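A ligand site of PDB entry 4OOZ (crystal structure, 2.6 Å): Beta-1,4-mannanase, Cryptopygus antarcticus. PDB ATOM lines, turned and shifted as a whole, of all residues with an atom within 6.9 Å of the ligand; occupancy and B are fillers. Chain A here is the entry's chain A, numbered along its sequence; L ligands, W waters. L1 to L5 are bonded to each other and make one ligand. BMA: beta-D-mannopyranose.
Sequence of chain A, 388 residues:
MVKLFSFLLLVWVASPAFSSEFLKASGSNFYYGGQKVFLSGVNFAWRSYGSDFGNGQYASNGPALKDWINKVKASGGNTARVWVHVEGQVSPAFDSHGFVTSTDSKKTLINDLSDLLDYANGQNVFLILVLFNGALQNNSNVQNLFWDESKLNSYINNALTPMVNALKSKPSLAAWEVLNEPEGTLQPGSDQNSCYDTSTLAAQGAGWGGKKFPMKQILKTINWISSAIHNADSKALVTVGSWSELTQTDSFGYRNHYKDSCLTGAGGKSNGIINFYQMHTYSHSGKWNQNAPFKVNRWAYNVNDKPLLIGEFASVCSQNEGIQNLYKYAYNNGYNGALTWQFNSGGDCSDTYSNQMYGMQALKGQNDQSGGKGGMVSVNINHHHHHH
Merely in contact with the ligand: Trp 147 (3.2 Å) and Ser 150 (3.5 Å). Hydrophobic or aromatic side chains within 4 Å of the ligand: Trp 147.
OD2 of Asp 148 is in hydrogen-bond range of O6 of BMA L1. The side-chain amide nitrogen (ND2) of Asn 144 lies within hydrogen-bond range of an oxygen (O2) of BMA L2 (3.0 Å). The side-chain amino group (NZ) of Lys 151 is in hydrogen-bond range of an oxygen (O2) of BMA L2 (3.0 Å). The side-chain amide nitrogen (NE2) of Gln 187 lies within hydrogen-bond range of an oxygen (O3) of BMA L4, 3.1 Å away.
The side-chain carboxylate (OD1) of Asp 148 sits at hydrogen-bond distance from the backbone NH (N) of Lys 151. The backbone NH (N) of Ser 150 lies within hydrogen-bond range of the side-chain carboxylate (OD1) of Asp 148. The backbone carbonyl oxygen (O) of Ser 140 sits close to the side-chain amide nitrogen (ND2) of Asn 144. The backbone carbonyl oxygen of His 97 is in hydrogen-bond range of the side-chain amino group of Lys 151 (3.3 Å). The side-chain amide nitrogen (NE2) of Gln 187 sits at hydrogen-bond distance from the backbone carbonyl oxygen (O) of Lys 211 (3.2 Å). The backbone NH (N) of Gln 187 is in hydrogen-bond range of the backbone carbonyl oxygen (O) of Phe 213 (2.7 Å).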
ATOM      1  N   HIS A  97      -3.359   8.361 -14.750  1.00  0.00           N
ATOM      2  CA  HIS A  97      -4.042   7.271 -14.075  1.00  0.00           C
ATOM      3  C   HIS A  97      -5.538   7.533 -13.900  1.00  0.00           C
ATOM      4  O   HIS A  97      -6.277   6.672 -13.433  1.00  0.00           O
ATOM      5  CB  HIS A  97      -3.410   6.995 -12.713  1.00  0.00           C
ATOM      6  CG  HIS A  97      -1.945   6.711 -12.785  1.00  0.00           C
ATOM      7  ND1 HIS A  97      -0.996   7.534 -12.225  1.00  0.00           N
ATOM      8  CD2 HIS A  97      -1.261   5.691 -13.375  1.00  0.00           C
ATOM      9  CE1 HIS A  97       0.210   7.032 -12.456  1.00  0.00           C
ATOM     10  NE2 HIS A  97       0.074   5.916 -13.142  1.00  0.00           N
ATOM     11  N   GLY A  98      -5.982   8.723 -14.280  1.00  0.00           N
ATOM     12  CA  GLY A  98      -7.384   9.078 -14.179  1.00  0.00           C
ATOM     13  C   GLY A  98      -7.730   9.803 -12.891  1.00  0.00           C
ATOM     14  O   GLY A  98      -8.901  10.014 -12.583  1.00  0.00           O
ATOM     15  N   PHE A  99      -6.708  10.163 -12.130  1.00  0.00           N
ATOM     16  CA  PHE A  99      -6.901  10.962 -10.923  1.00  0.00           C
ATOM     17  C   PHE A  99      -6.868  12.445 -11.285  1.00  0.00           C
ATOM     18  O   PHE A  99      -6.184  12.838 -12.220  1.00  0.00           O
ATOM     19  CB  PHE A  99      -5.834  10.628  -9.883  1.00  0.00           C
ATOM     20  CG  PHE A  99      -6.022   9.296  -9.221  1.00  0.00           C
ATOM     21  CD1 PHE A  99      -5.778   8.120  -9.910  1.00  0.00           C
ATOM     22  CD2 PHE A  99      -6.434   9.216  -7.898  1.00  0.00           C
ATOM     23  CE1 PHE A  99      -5.949   6.886  -9.299  1.00  0.00           C
ATOM     24  CE2 PHE A  99      -6.601   7.986  -7.278  1.00  0.00           C
ATOM     25  CZ  PHE A  99      -6.360   6.823  -7.985  1.00  0.00           C
ATOM     26  N   SER A 140     -13.759   8.755 -20.536  1.00  0.00           N
ATOM     27  CA  SER A 140     -13.504   7.579 -19.714  1.00  0.00           C
ATOM     28  C   SER A 140     -13.094   7.935 -18.281  1.00  0.00           C
ATOM     29  O   SER A 140     -13.310   7.158 -17.369  1.00  0.00           O
ATOM     30  CB  SER A 140     -12.432   6.708 -20.363  1.00  0.00           C
ATOM     31  OG  SER A 140     -12.894   6.148 -21.570  1.00  0.00           O
ATOM     32  N   GLN A 143     -16.357   9.198 -16.489  1.00  0.00           N
ATOM     33  CA  GLN A 143     -17.163   8.003 -16.294  1.00  0.00           C
ATOM     34  C   GLN A 143     -16.703   7.176 -15.106  1.00  0.00           C
ATOM     35  O   GLN A 143     -17.506   6.495 -14.466  1.00  0.00           O
ATOM     36  CB  GLN A 143     -17.143   7.131 -17.558  1.00  0.00           C
ATOM     37  CG  GLN A 143     -17.879   7.730 -18.741  1.00  0.00           C
ATOM     38  CD  GLN A 143     -17.669   6.935 -20.021  1.00  0.00           C
ATOM     39  OE1 GLN A 143     -17.331   5.753 -19.979  1.00  0.00           O
ATOM     40  NE2 GLN A 143     -17.842   7.599 -21.156  1.00  0.00           N
ATOM     41  N   ASN A 144     -15.413   7.238 -14.798  1.00  0.00           N
ATOM     42  CA  ASN A 144     -14.886   6.472 -13.679  1.00  0.00           C
ATOM     43  C   ASN A 144     -15.041   7.182 -12.344  1.00  0.00           C
ATOM     44  O   ASN A 144     -14.791   6.596 -11.290  1.00  0.00           O
ATOM     45  CB  ASN A 144     -13.415   6.119 -13.916  1.00  0.00           C
ATOM     46  CG  ASN A 144     -13.252   4.969 -14.890  1.00  0.00           C
ATOM     47  OD1 ASN A 144     -14.220   4.280 -15.212  1.00  0.00           O
ATOM     48  ND2 ASN A 144     -12.030   4.752 -15.347  1.00  0.00           N
ATOM     49  N   LEU A 145     -15.445   8.447 -12.384  1.00  0.00           N
ATOM     50  CA  LEU A 145     -15.711   9.199 -11.164  1.00  0.00           C
ATOM     51  C   LEU A 145     -16.924   8.637 -10.437  1.00  0.00           C
ATOM     52  O   LEU A 145     -17.091   8.847  -9.237  1.00  0.00           O
ATOM     53  CB  LEU A 145     -15.918  10.679 -11.462  1.00  0.00           C
ATOM     54  CG  LEU A 145     -14.676  11.477 -11.869  1.00  0.00           C
ATOM     55  CD1 LEU A 145     -15.032  12.944 -12.057  1.00  0.00           C
ATOM     56  CD2 LEU A 145     -13.576  11.325 -10.831  1.00  0.00           C
ATOM     57  N   PHE A 146     -17.771   7.920 -11.170  1.00  0.00           N
ATOM     58  CA  PHE A 146     -18.960   7.312 -10.606  1.00  0.00           C
ATOM     59  C   PHE A 146     -18.638   5.980  -9.936  1.00  0.00           C
ATOM     60  O   PHE A 146     -19.322   5.558  -9.011  1.00  0.00           O
ATOM     61  CB  PHE A 146     -20.026   7.087 -11.682  1.00  0.00           C
ATOM     62  CG  PHE A 146     -20.618   8.365 -12.219  1.00  0.00           C
ATOM     63  CD1 PHE A 146     -19.906   9.151 -13.107  1.00  0.00           C
ATOM     64  CD2 PHE A 146     -21.890   8.761 -11.834  1.00  0.00           C
ATOM     65  CE1 PHE A 146     -20.453  10.317 -13.595  1.00  0.00           C
ATOM     66  CE2 PHE A 146     -22.436   9.927 -12.322  1.00  0.00           C
ATOM     67  CZ  PHE A 146     -21.724  10.713 -13.210  1.00  0.00           C
ATOM     68  N   TRP A 147     -17.579   5.328 -10.421  1.00  0.00           N
ATOM     69  CA  TRP A 147     -17.239   3.993  -9.959  1.00  0.00           C
ATOM     70  C   TRP A 147     -16.116   3.986  -8.925  1.00  0.00           C
ATOM     71  O   TRP A 147     -16.219   3.313  -7.903  1.00  0.00           O
ATOM     72  CB  TRP A 147     -16.850   3.116 -11.149  1.00  0.00           C
ATOM     73  CG  TRP A 147     -17.990   2.796 -12.071  1.00  0.00           C
ATOM     74  CD1 TRP A 147     -18.288   3.419 -13.246  1.00  0.00           C
ATOM     75  CD2 TRP A 147     -18.964   1.763 -11.902  1.00  0.00           C
ATOM     76  NE1 TRP A 147     -19.400   2.846 -13.818  1.00  0.00           N
ATOM     77  CE2 TRP A 147     -19.829   1.822 -13.011  1.00  0.00           C
ATOM     78  CE3 TRP A 147     -19.194   0.793 -10.927  1.00  0.00           C
ATOM     79  CZ2 TRP A 147     -20.899   0.954 -13.169  1.00  0.00           C
ATOM     80  CZ3 TRP A 147     -20.251  -0.074 -11.081  1.00  0.00           C
ATOM     81  CH2 TRP A 147     -21.097   0.017 -12.192  1.00  0.00           C
ATOM     82  N   ASP A 148     -15.046   4.727  -9.199  1.00  0.00           N
ATOM     83  CA  ASP A 148     -13.893   4.744  -8.306  1.00  0.00           C
ATOM     84  C   ASP A 148     -14.037   5.846  -7.253  1.00  0.00           C
ATOM     85  O   ASP A 148     -14.179   7.020  -7.581  1.00  0.00           O
ATOM     86  CB  ASP A 148     -12.599   4.942  -9.102  1.00  0.00           C
ATOM     87  CG  ASP A 148     -11.352   4.624  -8.289  1.00  0.00           C
ATOM     88  OD1 ASP A 148     -11.194   5.200  -7.195  1.00  0.00           O
ATOM     89  OD2 ASP A 148     -10.543   3.795  -8.736  1.00  0.00           O
ATOM     90  N   GLU A 149     -13.993   5.432  -5.986  1.00  0.00           N
ATOM     91  CA  GLU A 149     -14.114   6.359  -4.874  1.00  0.00           C
ATOM     92  C   GLU A 149     -12.890   7.257  -4.737  1.00  0.00           C
ATOM     93  O   GLU A 149     -12.999   8.418  -4.373  1.00  0.00           O
ATOM     94  CB  GLU A 149     -14.356   5.612  -3.564  1.00  0.00           C
ATOM     95  CG  GLU A 149     -15.631   4.785  -3.537  1.00  0.00           C
ATOM     96  CD  GLU A 149     -15.941   4.237  -2.162  1.00  0.00           C
ATOM     97  OE1 GLU A 149     -15.318   4.688  -1.180  1.00  0.00           O
ATOM     98  OE2 GLU A 149     -16.817   3.348  -2.059  1.00  0.00           O
ATOM     99  N   SER A 150     -11.714   6.696  -5.033  1.00  0.00           N
ATOM    100  CA  SER A 150     -10.466   7.426  -4.867  1.00  0.00           C
ATOM    101  C   SER A 150     -10.275   8.477  -5.966  1.00  0.00           C
ATOM    102  O   SER A 150      -9.672   9.527  -5.738  1.00  0.00           O
ATOM    103  CB  SER A 150      -9.278   6.455  -4.870  1.00  0.00           C
ATOM    104  OG  SER A 150      -9.322   5.604  -5.999  1.00  0.00           O
ATOM    105  N   LYS A 151     -10.803   8.195  -7.152  1.00  0.00           N
ATOM    106  CA  LYS A 151     -10.762   9.156  -8.237  1.00  0.00           C
ATOM    107  C   LYS A 151     -11.765  10.276  -7.997  1.00  0.00           C
ATOM    108  O   LYS A 151     -11.480  11.456  -8.251  1.00  0.00           O
ATOM    109  CB  LYS A 151     -11.009   8.469  -9.575  1.00  0.00           C
ATOM    110  CG  LYS A 151      -9.937   7.436  -9.922  1.00  0.00           C
ATOM    111  CD  LYS A 151     -10.189   6.799 -11.273  1.00  0.00           C
ATOM    112  CE  LYS A 151      -9.018   5.935 -11.701  1.00  0.00           C
ATOM    113  NZ  LYS A 151      -9.251   5.368 -13.049  1.00  0.00           N
ATOM    114  N   GLN A 187     -28.108   3.193 -16.302  1.00  0.00           N
ATOM    115  CA  GLN A 187     -28.313   1.789 -16.608  1.00  0.00           C
ATOM    116  C   GLN A 187     -29.532   1.282 -15.845  1.00  0.00           C
ATOM    117  O   GLN A 187     -29.411   0.861 -14.689  1.00  0.00           O
ATOM    118  CB  GLN A 187     -27.072   0.969 -16.257  1.00  0.00           C
ATOM    119  CG  GLN A 187     -27.029  -0.408 -16.907  1.00  0.00           C
ATOM    120  CD  GLN A 187     -25.755  -1.168 -16.594  1.00  0.00           C
ATOM    121  OE1 GLN A 187     -25.504  -1.540 -15.445  1.00  0.00           O
ATOM    122  NE2 GLN A 187     -24.943  -1.403 -17.617  1.00  0.00           N
ATOM    123  N   LYS A 211     -26.102   3.194 -21.572  1.00  0.00           N
ATOM    124  CA  LYS A 211     -26.398   2.738 -20.217  1.00  0.00           C
ATOM    125  C   LYS A 211     -25.136   2.371 -19.448  1.00  0.00           C
ATOM    126  O   LYS A 211     -24.722   1.213 -19.422  1.00  0.00           O
ATOM    127  CB  LYS A 211     -27.363   1.557 -20.272  1.00  0.00           C
ATOM    128  CG  LYS A 211     -28.733   1.957 -20.802  1.00  0.00           C
ATOM    129  CD  LYS A 211     -29.537   0.778 -21.293  1.00  0.00           C
ATOM    130  CE  LYS A 211     -30.849   1.270 -21.904  1.00  0.00           C
ATOM    131  NZ  LYS A 211     -31.678   0.149 -22.414  1.00  0.00           N
ATOM    132  N   LYS A 212     -24.538   3.361 -18.796  1.00  0.00           N
ATOM    133  CA  LYS A 212     -23.268   3.175 -18.093  1.00  0.00           C
ATOM    134  C   LYS A 212     -23.450   3.037 -16.594  1.00  0.00           C
ATOM    135  O   LYS A 212     -22.916   2.104 -15.976  1.00  0.00           O
ATOM    136  CB  LYS A 212     -22.327   4.347 -18.383  1.00  0.00           C
ATOM    137  CG  LYS A 212     -22.314   4.801 -19.840  1.00  0.00           C
ATOM    138  CD  LYS A 212     -21.297   5.907 -20.059  1.00  0.00           C
ATOM    139  CE  LYS A 212     -21.451   6.500 -21.442  1.00  0.00           C
ATOM    140  NZ  LYS A 212     -21.545   5.438 -22.480  1.00  0.00           N
ATOM    141  N   PHE A 213     -24.185   3.964 -15.989  1.00  0.00           N
ATOM    142  CA  PHE A 213     -24.265   4.038 -14.534  1.00  0.00           C
ATOM    143  C   PHE A 213     -25.618   3.608 -13.969  1.00  0.00           C
ATOM    144  O   PHE A 213     -26.640   4.229 -14.251  1.00  0.00           O
ATOM    145  CB  PHE A 213     -23.973   5.468 -14.076  1.00  0.00           C
ATOM    146  CG  PHE A 213     -22.793   6.083 -14.751  1.00  0.00           C
ATOM    147  CD1 PHE A 213     -21.507   5.678 -14.437  1.00  0.00           C
ATOM    148  CD2 PHE A 213     -22.954   7.081 -15.700  1.00  0.00           C
ATOM    149  CE1 PHE A 213     -20.415   6.247 -15.055  1.00  0.00           C
ATOM    150  CE2 PHE A 213     -21.861   7.659 -16.323  1.00  0.00           C
ATOM    151  CZ  PHE A 213     -20.598   7.237 -16.000  1.00  0.00           C
ATOM    152  N   PRO A 214     -25.613   2.530 -13.172  1.00  0.00           N
ATOM    153  CA  PRO A 214     -26.800   2.161 -12.388  1.00  0.00           C
ATOM    154  C   PRO A 214     -27.157   3.257 -11.397  1.00  0.00           C
ATOM    155  O   PRO A 214     -26.269   3.986 -10.967  1.00  0.00           O
ATOM    156  CB  PRO A 214     -26.359   0.876 -11.667  1.00  0.00           C
ATOM    157  CG  PRO A 214     -24.866   0.891 -11.716  1.00  0.00           C
ATOM    158  CD  PRO A 214     -24.501   1.587 -12.988  1.00  0.00           C
HETATM  159  C1  BMA L   1      -4.933   2.182 -10.522  1.00  0.00           C
HETATM  160  C2  BMA L   1      -5.316   1.865 -11.966  1.00  0.00           C
HETATM  161  C3  BMA L   1      -6.733   2.372 -12.229  1.00  0.00           C
HETATM  162  C4  BMA L   1      -7.742   1.938 -11.141  1.00  0.00           C
HETATM  163  C5  BMA L   1      -7.170   2.203  -9.717  1.00  0.00           C
HETATM  164  C6  BMA L   1      -8.011   1.607  -8.602  1.00  0.00           C
HETATM  165  O1  BMA L   1      -3.695   1.566 -10.281  1.00  0.00           O
HETATM  166  O2  BMA L   1      -5.323   0.466 -12.190  1.00  0.00           O
HETATM  167  O3  BMA L   1      -7.200   1.945 -13.506  1.00  0.00           O
HETATM  168  O4  BMA L   1      -8.931   2.681 -11.338  1.00  0.00           O
HETATM  169  O5  BMA L   1      -5.858   1.627  -9.624  1.00  0.00           O
HETATM  170  O6  BMA L   1      -8.386   2.649  -7.709  1.00  0.00           O
HETATM  171  C1  BMA L   2     -10.086   1.820 -11.406  1.00  0.00           C
HETATM  172  C2  BMA L   2     -11.357   2.649 -11.557  1.00  0.00           C
HETATM  173  C3  BMA L   2     -12.566   1.743 -11.422  1.00  0.00           C
HETATM  174  C4  BMA L   2     -12.462   0.485 -12.307  1.00  0.00           C
HETATM  175  C5  BMA L   2     -11.046  -0.178 -12.259  1.00  0.00           C
HETATM  176  C6  BMA L   2     -10.829  -1.206 -13.340  1.00  0.00           C
HETATM  177  O2  BMA L   2     -11.426   3.250 -12.839  1.00  0.00           O
HETATM  178  O3  BMA L   2     -13.755   2.435 -11.730  1.00  0.00           O
HETATM  179  O4  BMA L   2     -13.426  -0.446 -11.835  1.00  0.00           O
HETATM  180  O5  BMA L   2     -10.011   0.826 -12.394  1.00  0.00           O
HETATM  181  O6  BMA L   2     -11.474  -2.410 -12.948  1.00  0.00           O
HETATM  182  C1  BMA L   3     -14.401  -0.764 -12.844  1.00  0.00           C
HETATM  183  C2  BMA L   3     -15.492  -1.613 -12.213  1.00  0.00           C
HETATM  184  C3  BMA L   3     -16.519  -2.023 -13.269  1.00  0.00           C
HETATM  185  C4  BMA L   3     -16.948  -0.846 -14.201  1.00  0.00           C
HETATM  186  C5  BMA L   3     -15.713  -0.022 -14.643  1.00  0.00           C
HETATM  187  C6  BMA L   3     -16.067   1.225 -15.426  1.00  0.00           C
HETATM  188  O2  BMA L   3     -16.181  -0.858 -11.237  1.00  0.00           O
HETATM  189  O3  BMA L   3     -17.648  -2.612 -12.647  1.00  0.00           O
HETATM  190  O4  BMA L   3     -17.590  -1.337 -15.377  1.00  0.00           O
HETATM  191  O5  BMA L   3     -14.945   0.356 -13.496  1.00  0.00           O
HETATM  192  O6  BMA L   3     -16.091   0.885 -16.807  1.00  0.00           O
HETATM  193  C1  BMA L   4     -18.993  -1.608 -15.186  1.00  0.00           C
HETATM  194  C2  BMA L   4     -19.767  -1.291 -16.483  1.00  0.00           C
HETATM  195  C3  BMA L   4     -21.211  -1.822 -16.430  1.00  0.00           C
HETATM  196  C4  BMA L   4     -21.278  -3.254 -15.877  1.00  0.00           C
HETATM  197  C5  BMA L   4     -20.558  -3.298 -14.525  1.00  0.00           C
HETATM  198  C6  BMA L   4     -20.580  -4.670 -13.866  1.00  0.00           C
HETATM  199  O2  BMA L   4     -19.142  -1.906 -17.602  1.00  0.00           O
HETATM  200  O3  BMA L   4     -21.831  -1.761 -17.705  1.00  0.00           O
HETATM  201  O4  BMA L   4     -22.636  -3.648 -15.718  1.00  0.00           O
HETATM  202  O5  BMA L   4     -19.198  -2.937 -14.743  1.00  0.00           O
HETATM  203  O6  BMA L   4     -20.488  -4.490 -12.459  1.00  0.00           O
HETATM  204  C1  BMA L   5     -22.944  -4.775 -16.558  1.00  0.00           C
HETATM  205  C2  BMA L   5     -23.864  -5.750 -15.773  1.00  0.00           C
HETATM  206  C3  BMA L   5     -24.397  -6.858 -16.694  1.00  0.00           C
HETATM  207  C4  BMA L   5     -24.913  -6.301 -18.019  1.00  0.00           C
HETATM  208  C5  BMA L   5     -23.807  -5.481 -18.680  1.00  0.00           C
HETATM  209  C6  BMA L   5     -24.223  -4.901 -20.020  1.00  0.00           C
HETATM  210  O2  BMA L   5     -24.991  -5.066 -15.256  1.00  0.00           O
HETATM  211  O3  BMA L   5     -25.426  -7.609 -16.049  1.00  0.00           O
HETATM  212  O4  BMA L   5     -25.310  -7.356 -18.878  1.00  0.00           O
HETATM  213  O5  BMA L   5     -23.491  -4.379 -17.804  1.00  0.00           O
HETATM  214  O6  BMA L   5     -23.661  -3.609 -20.140  1.00  0.00           O
HETATM  215  O   HOH W   1      -2.927   4.592  -9.651  1.00  0.00           O
HETATM  216  O   HOH W   2      -9.593   1.190  -5.557  1.00  0.00           O
